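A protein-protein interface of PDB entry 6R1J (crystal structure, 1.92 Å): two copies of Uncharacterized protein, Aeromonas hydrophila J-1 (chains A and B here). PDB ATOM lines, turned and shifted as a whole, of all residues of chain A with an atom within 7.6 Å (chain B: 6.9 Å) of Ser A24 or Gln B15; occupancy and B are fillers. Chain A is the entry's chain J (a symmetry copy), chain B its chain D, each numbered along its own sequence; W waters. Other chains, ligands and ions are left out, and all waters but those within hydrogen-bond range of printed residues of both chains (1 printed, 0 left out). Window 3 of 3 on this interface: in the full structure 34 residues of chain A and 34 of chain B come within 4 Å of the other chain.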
ATOM      1  N   THR A  19     -13.916  -1.656 -19.124  1.00  0.00           N
ATOM      2  CA  THR A  19     -14.799  -2.269 -18.123  1.00  0.00           C
ATOM      3  C   THR A  19     -16.130  -1.492 -18.065  1.00  0.00           C
ATOM      4  O   THR A  19     -17.193  -2.157 -17.983  1.00  0.00           O
ATOM      5  CB  THR A  19     -14.074  -2.396 -16.786  1.00  0.00           C
ATOM      6  OG1 THR A  19     -12.930  -3.203 -17.053  1.00  0.00           O
ATOM      7  CG2 THR A  19     -14.925  -3.084 -15.750  1.00  0.00           C
ATOM      8  N   ILE A  20     -16.075  -0.168 -18.111  1.00  0.00           N
ATOM      9  CA  ILE A  20     -17.296   0.678 -18.079  1.00  0.00           C
ATOM     10  C   ILE A  20     -18.175   0.351 -19.290  1.00  0.00           C
ATOM     11  O   ILE A  20     -19.401   0.276 -19.110  1.00  0.00           O
ATOM     12  CB  ILE A  20     -16.924   2.157 -17.991  1.00  0.00           C
ATOM     13  CG1 ILE A  20     -16.383   2.491 -16.595  1.00  0.00           C
ATOM     14  CG2 ILE A  20     -18.126   3.009 -18.348  1.00  0.00           C
ATOM     15  CD1 ILE A  20     -15.788   3.858 -16.465  1.00  0.00           C
ATOM     16  N   GLN A  21     -17.589   0.060 -20.450  1.00  0.00           N
ATOM     17  CA  GLN A  21     -18.414  -0.214 -21.658  1.00  0.00           C
ATOM     18  C   GLN A  21     -19.088  -1.592 -21.564  1.00  0.00           C
ATOM     19  O   GLN A  21     -20.058  -1.772 -22.281  1.00  0.00           O
ATOM     20  CB  GLN A  21     -17.605  -0.119 -22.949  1.00  0.00           C
ATOM     21  CG  GLN A  21     -16.982   1.246 -23.169  1.00  0.00           C
ATOM     22  CD  GLN A  21     -17.942   2.408 -23.232  1.00  0.00           C
ATOM     23  OE1 GLN A  21     -19.164   2.243 -23.269  1.00  0.00           O
ATOM     24  NE2 GLN A  21     -17.389   3.616 -23.195  1.00  0.00           N
ATOM     25  N   SER A  22     -18.631  -2.512 -20.704  1.00  0.00           N
ATOM     26  CA  SER A  22     -19.119  -3.895 -20.637  1.00  0.00           C
ATOM     27  C   SER A  22     -20.495  -3.950 -19.968  1.00  0.00           C
ATOM     28  O   SER A  22     -21.101  -4.992 -20.055  1.00  0.00           O
ATOM     29  CB  SER A  22     -18.117  -4.817 -19.959  1.00  0.00           C
ATOM     30  OG  SER A  22     -18.146  -4.646 -18.561  1.00  0.00           O
ATOM     31  N   PHE A  23     -20.925  -2.886 -19.295  1.00  0.00           N
ATOM     32  CA  PHE A  23     -22.179  -2.851 -18.525  1.00  0.00           C
ATOM     33  C   PHE A  23     -23.354  -2.537 -19.455  1.00  0.00           C
ATOM     34  O   PHE A  23     -23.258  -1.626 -20.269  1.00  0.00           O
ATOM     35  CB  PHE A  23     -22.085  -1.839 -17.385  1.00  0.00           C
ATOM     36  CG  PHE A  23     -21.285  -2.312 -16.180  1.00  0.00           C
ATOM     37  CD1 PHE A  23     -19.904  -2.166 -16.137  1.00  0.00           C
ATOM     38  CD2 PHE A  23     -21.916  -2.911 -15.098  1.00  0.00           C
ATOM     39  CE1 PHE A  23     -19.186  -2.577 -15.018  1.00  0.00           C
ATOM     40  CE2 PHE A  23     -21.189  -3.363 -13.999  1.00  0.00           C
ATOM     41  CZ  PHE A  23     -19.827  -3.175 -13.951  1.00  0.00           C
ATOM     42  N   SER A  24     -24.428  -3.310 -19.333  1.00  0.00           N
ATOM     43  CA  SER A  24     -25.679  -3.081 -20.093  1.00  0.00           C
ATOM     44  C   SER A  24     -26.865  -2.999 -19.126  1.00  0.00           C
ATOM     45  O   SER A  24     -26.760  -3.404 -17.921  1.00  0.00           O
ATOM     46  CB  SER A  24     -25.837  -4.143 -21.147  1.00  0.00           C
ATOM     47  OG  SER A  24     -25.925  -5.434 -20.558  1.00  0.00           O
ATOM     48  N   GLY A  25     -27.962  -2.430 -19.610  1.00  0.00           N
ATOM     49  CA  GLY A  25     -29.233  -2.419 -18.870  1.00  0.00           C
ATOM     50  C   GLY A  25     -29.215  -1.387 -17.780  1.00  0.00           C
ATOM     51  O   GLY A  25     -29.944  -1.561 -16.827  1.00  0.00           O
ATOM     52  N   LEU A  26     -28.372  -0.364 -17.899  1.00  0.00           N
ATOM     53  CA  LEU A  26     -28.280   0.680 -16.854  1.00  0.00           C
ATOM     54  C   LEU A  26     -29.050   1.916 -17.311  1.00  0.00           C
ATOM     55  O   LEU A  26     -29.367   2.081 -18.485  1.00  0.00           O
ATOM     56  CB  LEU A  26     -26.801   0.961 -16.538  1.00  0.00           C
ATOM     57  CG  LEU A  26     -26.063  -0.179 -15.832  1.00  0.00           C
ATOM     58  CD1 LEU A  26     -24.580   0.151 -15.668  1.00  0.00           C
ATOM     59  CD2 LEU A  26     -26.690  -0.496 -14.466  1.00  0.00           C
ATOM     60  N   PRO A  27     -29.396   2.806 -16.378  1.00  0.00           N
ATOM     61  CA  PRO A  27     -30.134   4.013 -16.728  1.00  0.00           C
ATOM     62  C   PRO A  27     -29.329   5.073 -17.471  1.00  0.00           C
ATOM     63  O   PRO A  27     -28.094   4.967 -17.598  1.00  0.00           O
ATOM     64  CB  PRO A  27     -30.590   4.579 -15.378  1.00  0.00           C
ATOM     65  CG  PRO A  27     -29.625   3.986 -14.367  1.00  0.00           C
ATOM     66  CD  PRO A  27     -29.246   2.634 -14.920  1.00  0.00           C
ATOM     67  N   VAL A  31     -25.380   5.572 -19.158  1.00  0.00           N
ATOM     68  CA  VAL A  31     -25.115   5.758 -20.605  1.00  0.00           C
ATOM     69  C   VAL A  31     -24.410   7.102 -20.826  1.00  0.00           C
ATOM     70  O   VAL A  31     -23.525   7.153 -21.688  1.00  0.00           O
ATOM     71  CB  VAL A  31     -26.403   5.619 -21.440  1.00  0.00           C
ATOM     72  CG1 VAL A  31     -26.108   5.857 -22.906  1.00  0.00           C
ATOM     73  CG2 VAL A  31     -27.005   4.248 -21.261  1.00  0.00           C
ATOM     74  N   GLN A  34     -20.771   6.374 -20.016  1.00  0.00           N
ATOM     75  CA  GLN A  34     -20.235   5.438 -21.049  1.00  0.00           C
ATOM     76  C   GLN A  34     -19.854   6.252 -22.288  1.00  0.00           C
ATOM     77  O   GLN A  34     -18.751   6.025 -22.873  1.00  0.00           O
ATOM     78  CB  GLN A  34     -21.244   4.347 -21.425  1.00  0.00           C
ATOM     79  CG  GLN A  34     -21.423   3.269 -20.349  1.00  0.00           C
ATOM     80  CD  GLN A  34     -22.337   2.141 -20.767  1.00  0.00           C
ATOM     81  OE1 GLN A  34     -23.349   2.388 -21.406  1.00  0.00           O
ATOM     82  NE2 GLN A  34     -22.001   0.897 -20.429  1.00  0.00           N
ATOM     83  N   GLY A 192     -30.272  -7.574  -7.725  1.00  0.00           N
ATOM     84  CA  GLY A 192     -29.368  -7.694  -8.894  1.00  0.00           C
ATOM     85  C   GLY A 192     -29.060  -6.329  -9.516  1.00  0.00           C
ATOM     86  O   GLY A 192     -27.878  -6.065  -9.881  1.00  0.00           O
ATOM     87  N   ARG A 196     -25.418  -4.565  -9.705  1.00  0.00           N
ATOM     88  CA  ARG A 196     -24.863  -4.136 -11.005  1.00  0.00           C
ATOM     89  C   ARG A 196     -24.548  -2.649 -10.963  1.00  0.00           C
ATOM     90  O   ARG A 196     -23.471  -2.237 -11.450  1.00  0.00           O
ATOM     91  CB  ARG A 196     -25.889  -4.416 -12.093  1.00  0.00           C
ATOM     92  CG  ARG A 196     -25.374  -4.173 -13.489  1.00  0.00           C
ATOM     93  CD  ARG A 196     -26.442  -4.560 -14.485  1.00  0.00           C
ATOM     94  NE  ARG A 196     -26.777  -5.981 -14.460  1.00  0.00           N
ATOM     95  CZ  ARG A 196     -27.354  -6.632 -15.484  1.00  0.00           C
ATOM     96  NH1 ARG A 196     -27.627  -5.991 -16.614  1.00  0.00           N
ATOM     97  NH2 ARG A 196     -27.608  -7.930 -15.400  1.00  0.00           N
ATOM     98  N   PHE A 200     -20.877  -0.838 -11.354  1.00  0.00           N
ATOM     99  CA  PHE A 200     -20.645   0.215 -12.373  1.00  0.00           C
ATOM    100  C   PHE A 200     -20.083   1.483 -11.728  1.00  0.00           C
ATOM    101  O   PHE A 200     -19.129   2.089 -12.223  1.00  0.00           O
ATOM    102  CB  PHE A 200     -21.962   0.512 -13.103  1.00  0.00           C
ATOM    103  CG  PHE A 200     -21.799   1.561 -14.148  1.00  0.00           C
ATOM    104  CD1 PHE A 200     -21.385   1.224 -15.430  1.00  0.00           C
ATOM    105  CD2 PHE A 200     -22.134   2.882 -13.881  1.00  0.00           C
ATOM    106  CE1 PHE A 200     -21.266   2.210 -16.407  1.00  0.00           C
ATOM    107  CE2 PHE A 200     -22.016   3.855 -14.867  1.00  0.00           C
ATOM    108  CZ  PHE A 200     -21.587   3.520 -16.129  1.00  0.00           C
ATOM    109  N   ILE B  10     -28.979 -16.823 -13.951  1.00  0.00           N
ATOM    110  CA  ILE B  10     -28.315 -17.020 -15.273  1.00  0.00           C
ATOM    111  C   ILE B  10     -27.999 -15.657 -15.890  1.00  0.00           C
ATOM    112  O   ILE B  10     -26.823 -15.428 -16.208  1.00  0.00           O
ATOM    113  CB  ILE B  10     -29.160 -17.905 -16.197  1.00  0.00           C
ATOM    114  CG1 ILE B  10     -29.140 -19.352 -15.712  1.00  0.00           C
ATOM    115  CG2 ILE B  10     -28.699 -17.777 -17.636  1.00  0.00           C
ATOM    116  CD1 ILE B  10     -30.180 -20.246 -16.360  1.00  0.00           C
ATOM    117  N   ALA B  11     -29.000 -14.782 -16.022  1.00  0.00           N
ATOM    118  CA  ALA B  11     -28.864 -13.441 -16.622  1.00  0.00           C
ATOM    119  C   ALA B  11     -27.798 -12.629 -15.889  1.00  0.00           C
ATOM    120  O   ALA B  11     -27.016 -11.949 -16.559  1.00  0.00           O
ATOM    121  CB  ALA B  11     -30.186 -12.714 -16.569  1.00  0.00           C
ATOM    122  N   ASN B  12     -27.819 -12.623 -14.558  1.00  0.00           N
ATOM    123  CA  ASN B  12     -26.848 -11.820 -13.775  1.00  0.00           C
ATOM    124  C   ASN B  12     -25.460 -12.436 -13.984  1.00  0.00           C
ATOM    125  O   ASN B  12     -24.506 -11.655 -14.102  1.00  0.00           O
ATOM    126  CB  ASN B  12     -27.270 -11.707 -12.317  1.00  0.00           C
ATOM    127  CG  ASN B  12     -28.580 -10.954 -12.157  1.00  0.00           C
ATOM    128  OD1 ASN B  12     -28.843 -10.005 -12.886  1.00  0.00           O
ATOM    129  ND2 ASN B  12     -29.381 -11.343 -11.188  1.00  0.00           N
ATOM    130  N   MET B  13     -25.377 -13.762 -14.125  1.00  0.00           N
ATOM    131  CA  MET B  13     -24.083 -14.461 -14.341  1.00  0.00           C
ATOM    132  C   MET B  13     -23.511 -14.036 -15.694  1.00  0.00           C
ATOM    133  O   MET B  13     -22.309 -13.756 -15.730  1.00  0.00           O
ATOM    134  CB  MET B  13     -24.200 -15.980 -14.221  1.00  0.00           C
ATOM    135  CG  MET B  13     -24.220 -16.400 -12.741  1.00  0.00           C
ATOM    136  SD  MET B  13     -24.683 -18.111 -12.428  1.00  0.00           S
ATOM    137  CE  MET B  13     -23.177 -18.949 -12.890  1.00  0.00           C
ATOM    138  N   GLN B  14     -24.341 -13.897 -16.725  1.00  0.00           N
ATOM    139  CA  GLN B  14     -23.888 -13.479 -18.075  1.00  0.00           C
ATOM    140  C   GLN B  14     -23.304 -12.055 -18.031  1.00  0.00           C
ATOM    141  O   GLN B  14     -22.184 -11.850 -18.564  1.00  0.00           O
ATOM    142  CB  GLN B  14     -25.016 -13.713 -19.077  1.00  0.00           C
ATOM    143  CG  GLN B  14     -25.269 -15.200 -19.311  1.00  0.00           C
ATOM    144  CD  GLN B  14     -26.631 -15.533 -19.878  1.00  0.00           C
ATOM    145  OE1 GLN B  14     -27.567 -14.751 -19.802  1.00  0.00           O
ATOM    146  NE2 GLN B  14     -26.780 -16.744 -20.384  1.00  0.00           N
ATOM    147  N   GLN B  15     -23.964 -11.107 -17.367  1.00  0.00           N
ATOM    148  CA  GLN B  15     -23.472  -9.703 -17.277  1.00  0.00           C
ATOM    149  C   GLN B  15     -22.144  -9.684 -16.525  1.00  0.00           C
ATOM    150  O   GLN B  15     -21.197  -9.019 -16.992  1.00  0.00           O
ATOM    151  CB  GLN B  15     -24.483  -8.808 -16.545  1.00  0.00           C
ATOM    152  CG  GLN B  15     -23.925  -7.463 -16.070  1.00  0.00           C
ATOM    153  CD  GLN B  15     -23.570  -6.504 -17.190  1.00  0.00           C
ATOM    154  OE1 GLN B  15     -24.301  -5.550 -17.498  1.00  0.00           O
ATOM    155  NE2 GLN B  15     -22.428  -6.742 -17.807  1.00  0.00           N
ATOM    156  N   ALA B  16     -22.062 -10.350 -15.374  1.00  0.00           N
ATOM    157  CA  ALA B  16     -20.804 -10.331 -14.603  1.00  0.00           C
ATOM    158  C   ALA B  16     -19.690 -10.922 -15.490  1.00  0.00           C
ATOM    159  O   ALA B  16     -18.623 -10.325 -15.558  1.00  0.00           O
ATOM    160  CB  ALA B  16     -20.949 -11.020 -13.266  1.00  0.00           C
ATOM    161  N   GLU B  17     -19.951 -12.009 -16.208  1.00  0.00           N
ATOM    162  CA  GLU B  17     -18.927 -12.660 -17.073  1.00  0.00           C
ATOM    163  C   GLU B  17     -18.394 -11.679 -18.140  1.00  0.00           C
ATOM    164  O   GLU B  17     -17.192 -11.635 -18.304  1.00  0.00           O
ATOM    165  CB  GLU B  17     -19.477 -13.975 -17.631  1.00  0.00           C
ATOM    166  CG  GLU B  17     -18.417 -14.841 -18.283  1.00  0.00           C
ATOM    167  CD  GLU B  17     -18.149 -14.514 -19.738  1.00  0.00           C
ATOM    168  OE1 GLU B  17     -18.898 -13.677 -20.296  1.00  0.00           O
ATOM    169  OE2 GLU B  17     -17.217 -15.122 -20.299  1.00  0.00           O
ATOM    170  N   ALA B  18     -19.218 -10.860 -18.791  1.00  0.00           N
ATOM    171  CA  ALA B  18     -18.741  -9.888 -19.805  1.00  0.00           C
ATOM    172  C   ALA B  18     -17.796  -8.870 -19.159  1.00  0.00           C
ATOM    173  O   ALA B  18     -16.712  -8.533 -19.731  1.00  0.00           O
ATOM    174  CB  ALA B  18     -19.917  -9.183 -20.440  1.00  0.00           C
ATOM    175  N   THR B  19     -18.180  -8.397 -17.979  1.00  0.00           N
ATOM    176  CA  THR B  19     -17.419  -7.413 -17.184  1.00  0.00           C
ATOM    177  C   THR B  19     -16.129  -8.074 -16.705  1.00  0.00           C
ATOM    178  O   THR B  19     -15.071  -7.441 -16.761  1.00  0.00           O
ATOM    179  CB  THR B  19     -18.283  -6.888 -16.041  1.00  0.00           C
ATOM    180  OG1 THR B  19     -19.430  -6.289 -16.645  1.00  0.00           O
ATOM    181  CG2 THR B  19     -17.538  -5.868 -15.218  1.00  0.00           C
ATOM    182  N   ILE B  20     -16.228  -9.301 -16.223  1.00  0.00           N
ATOM    183  CA  ILE B  20     -15.040 -10.075 -15.770  1.00  0.00           C
ATOM    184  C   ILE B  20     -14.024 -10.234 -16.930  1.00  0.00           C
ATOM    185  O   ILE B  20     -12.809 -10.063 -16.662  1.00  0.00           O
ATOM    186  CB  ILE B  20     -15.526 -11.390 -15.149  1.00  0.00           C
ATOM    187  CG1 ILE B  20     -16.040 -11.128 -13.722  1.00  0.00           C
ATOM    188  CG2 ILE B  20     -14.433 -12.444 -15.163  1.00  0.00           C
ATOM    189  CD1 ILE B  20     -16.899 -12.246 -13.171  1.00  0.00           C
ATOM    190  N   VAL B  41     -20.371 -19.940 -18.492  1.00  0.00           N
ATOM    191  CA  VAL B  41     -21.342 -19.272 -19.402  1.00  0.00           C
ATOM    192  C   VAL B  41     -21.506 -20.033 -20.732  1.00  0.00           C
ATOM    193  O   VAL B  41     -22.677 -20.144 -21.186  1.00  0.00           O
ATOM    194  CB  VAL B  41     -20.983 -17.792 -19.619  1.00  0.00           C
ATOM    195  CG1 VAL B  41     -21.777 -17.159 -20.758  1.00  0.00           C
ATOM    196  CG2 VAL B  41     -21.187 -17.034 -18.315  1.00  0.00           C
ATOM    197  N   GLN B 203     -16.597  -7.958  -9.006  1.00  0.00           N
ATOM    198  CA  GLN B 203     -17.328  -8.676 -10.068  1.00  0.00           C
ATOM    199  C   GLN B 203     -17.322 -10.181  -9.822  1.00  0.00           C
ATOM    200  O   GLN B 203     -18.396 -10.823 -10.013  1.00  0.00           O
ATOM    201  CB  GLN B 203     -16.731  -8.296 -11.423  1.00  0.00           C
ATOM    202  CG  GLN B 203     -16.876  -6.831 -11.748  1.00  0.00           C
ATOM    203  CD  GLN B 203     -18.339  -6.465 -11.775  1.00  0.00           C
ATOM    204  OE1 GLN B 203     -19.140  -7.029 -12.506  1.00  0.00           O
ATOM    205  NE2 GLN B 203     -18.701  -5.567 -10.908  1.00  0.00           N
ATOM    206  N   PHE B 207     -20.516 -12.529  -9.215  1.00  0.00           N
ATOM    207  CA  PHE B 207     -20.730 -13.739 -10.048  1.00  0.00           C
ATOM    208  C   PHE B 207     -20.974 -14.940  -9.138  1.00  0.00           C
ATOM    209  O   PHE B 207     -21.925 -15.701  -9.336  1.00  0.00           O
ATOM    210  CB  PHE B 207     -19.521 -14.037 -10.930  1.00  0.00           C
ATOM    211  CG  PHE B 207     -19.754 -15.170 -11.892  1.00  0.00           C
ATOM    212  CD1 PHE B 207     -19.526 -16.476 -11.521  1.00  0.00           C
ATOM    213  CD2 PHE B 207     -20.185 -14.900 -13.179  1.00  0.00           C
ATOM    214  CE1 PHE B 207     -19.733 -17.506 -12.419  1.00  0.00           C
ATOM    215  CE2 PHE B 207     -20.397 -15.930 -14.076  1.00  0.00           C
ATOM    216  CZ  PHE B 207     -20.170 -17.230 -13.693  1.00  0.00           C
HETATM  217  O   HOH W   1     -29.560  -7.064 -12.699  1.00  0.00           O
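Of the 14 printed residues of chain A, 5 touch a printed residue of chain B. Hydrophobic or aromatic side chains of chain A that line the printed part of chain B: Phe A23. Printed residues of chain B that touch a printed residue of chain A: Asn B12, Gln B15, Ala B18 and Thr B19. Among the printed residues, no Asp or Glu carboxylate lies within 4 Å of a Lys or Arg side-chain nitrogen of the other chain.
Ser A24 touches just one residue of chain B: Gln B15. Of the printed residues of chain A, Gln B15 touches Ser A22, Phe A23, Ser A24 and Arg A196. Of the printed residues of chain B, Arg A196 touches Asn B12 and Gln B15. Of the printed residues of chain B, Ser A22 touches Gln B15, Ala B18 and Thr B19. Printed residues of chain A within 4 Å of Ala B18: Ser A22.
Water W1 lies within hydrogen-bond range of the side-chain amide oxygen of Asn B12 (3.0 Å), the backbone carbonyl oxygen of Gly A192 (3.4 Å) and the guanidinium group of Arg A196 (3.4 Å).
Thr A19 touches Thr B19. O of Ala B18 touches CB of Ser A22, at 3.98 Å. Phe A23 touches Gln B15. Phe A23 touches Thr B19.
The guanidinium group (NH1) of Arg A196 is in hydrogen-bond range of the side-chain amide oxygen (OE1) of Gln B15 (3.5 Å). OE1 of Gln B15 lies within hydrogen-bond range of N of Ser A24. The side-chain amide nitrogen of Gln B15 lies within hydrogen-bond range of the backbone carbonyl oxygen of Ser A22, at 3.1 Å. The guanidinium group (NH2) of Arg A196 is in hydrogen-bond range of the side-chain amide oxygen (OD1) of Asn B12 (3.5 Å). The side-chain hydroxyl (OG1) of Thr B19 sits at hydrogen-bond distance from the side-chain hydroxyl (OG) of Ser A22 (2.8 Å).
Thr A19 touches its own counterpart, Thr B19. 2 positions are printed for both chains. Of the 9 pairs that touch across the chains among the printed residues, 1 has its exchanged pair printed and touching as well.
The side-chain amide nitrogen of Gln A34 is in hydrogen-bond range of the backbone carbonyl oxygen of Phe A23 (2.8 Å). The side-chain amide nitrogen (NE2) of Gln B15 is in hydrogen-bond range of the side-chain hydroxyl (OG1) of Thr B19. The backbone carbonyl oxygen (O) of Thr A19 lies within hydrogen-bond range of the side-chain hydroxyl (OG) of Ser A22, 2.7 Å away. O of Ser A24 lies within hydrogen-bond range of NH1 of Arg A196 (3.0 Å).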
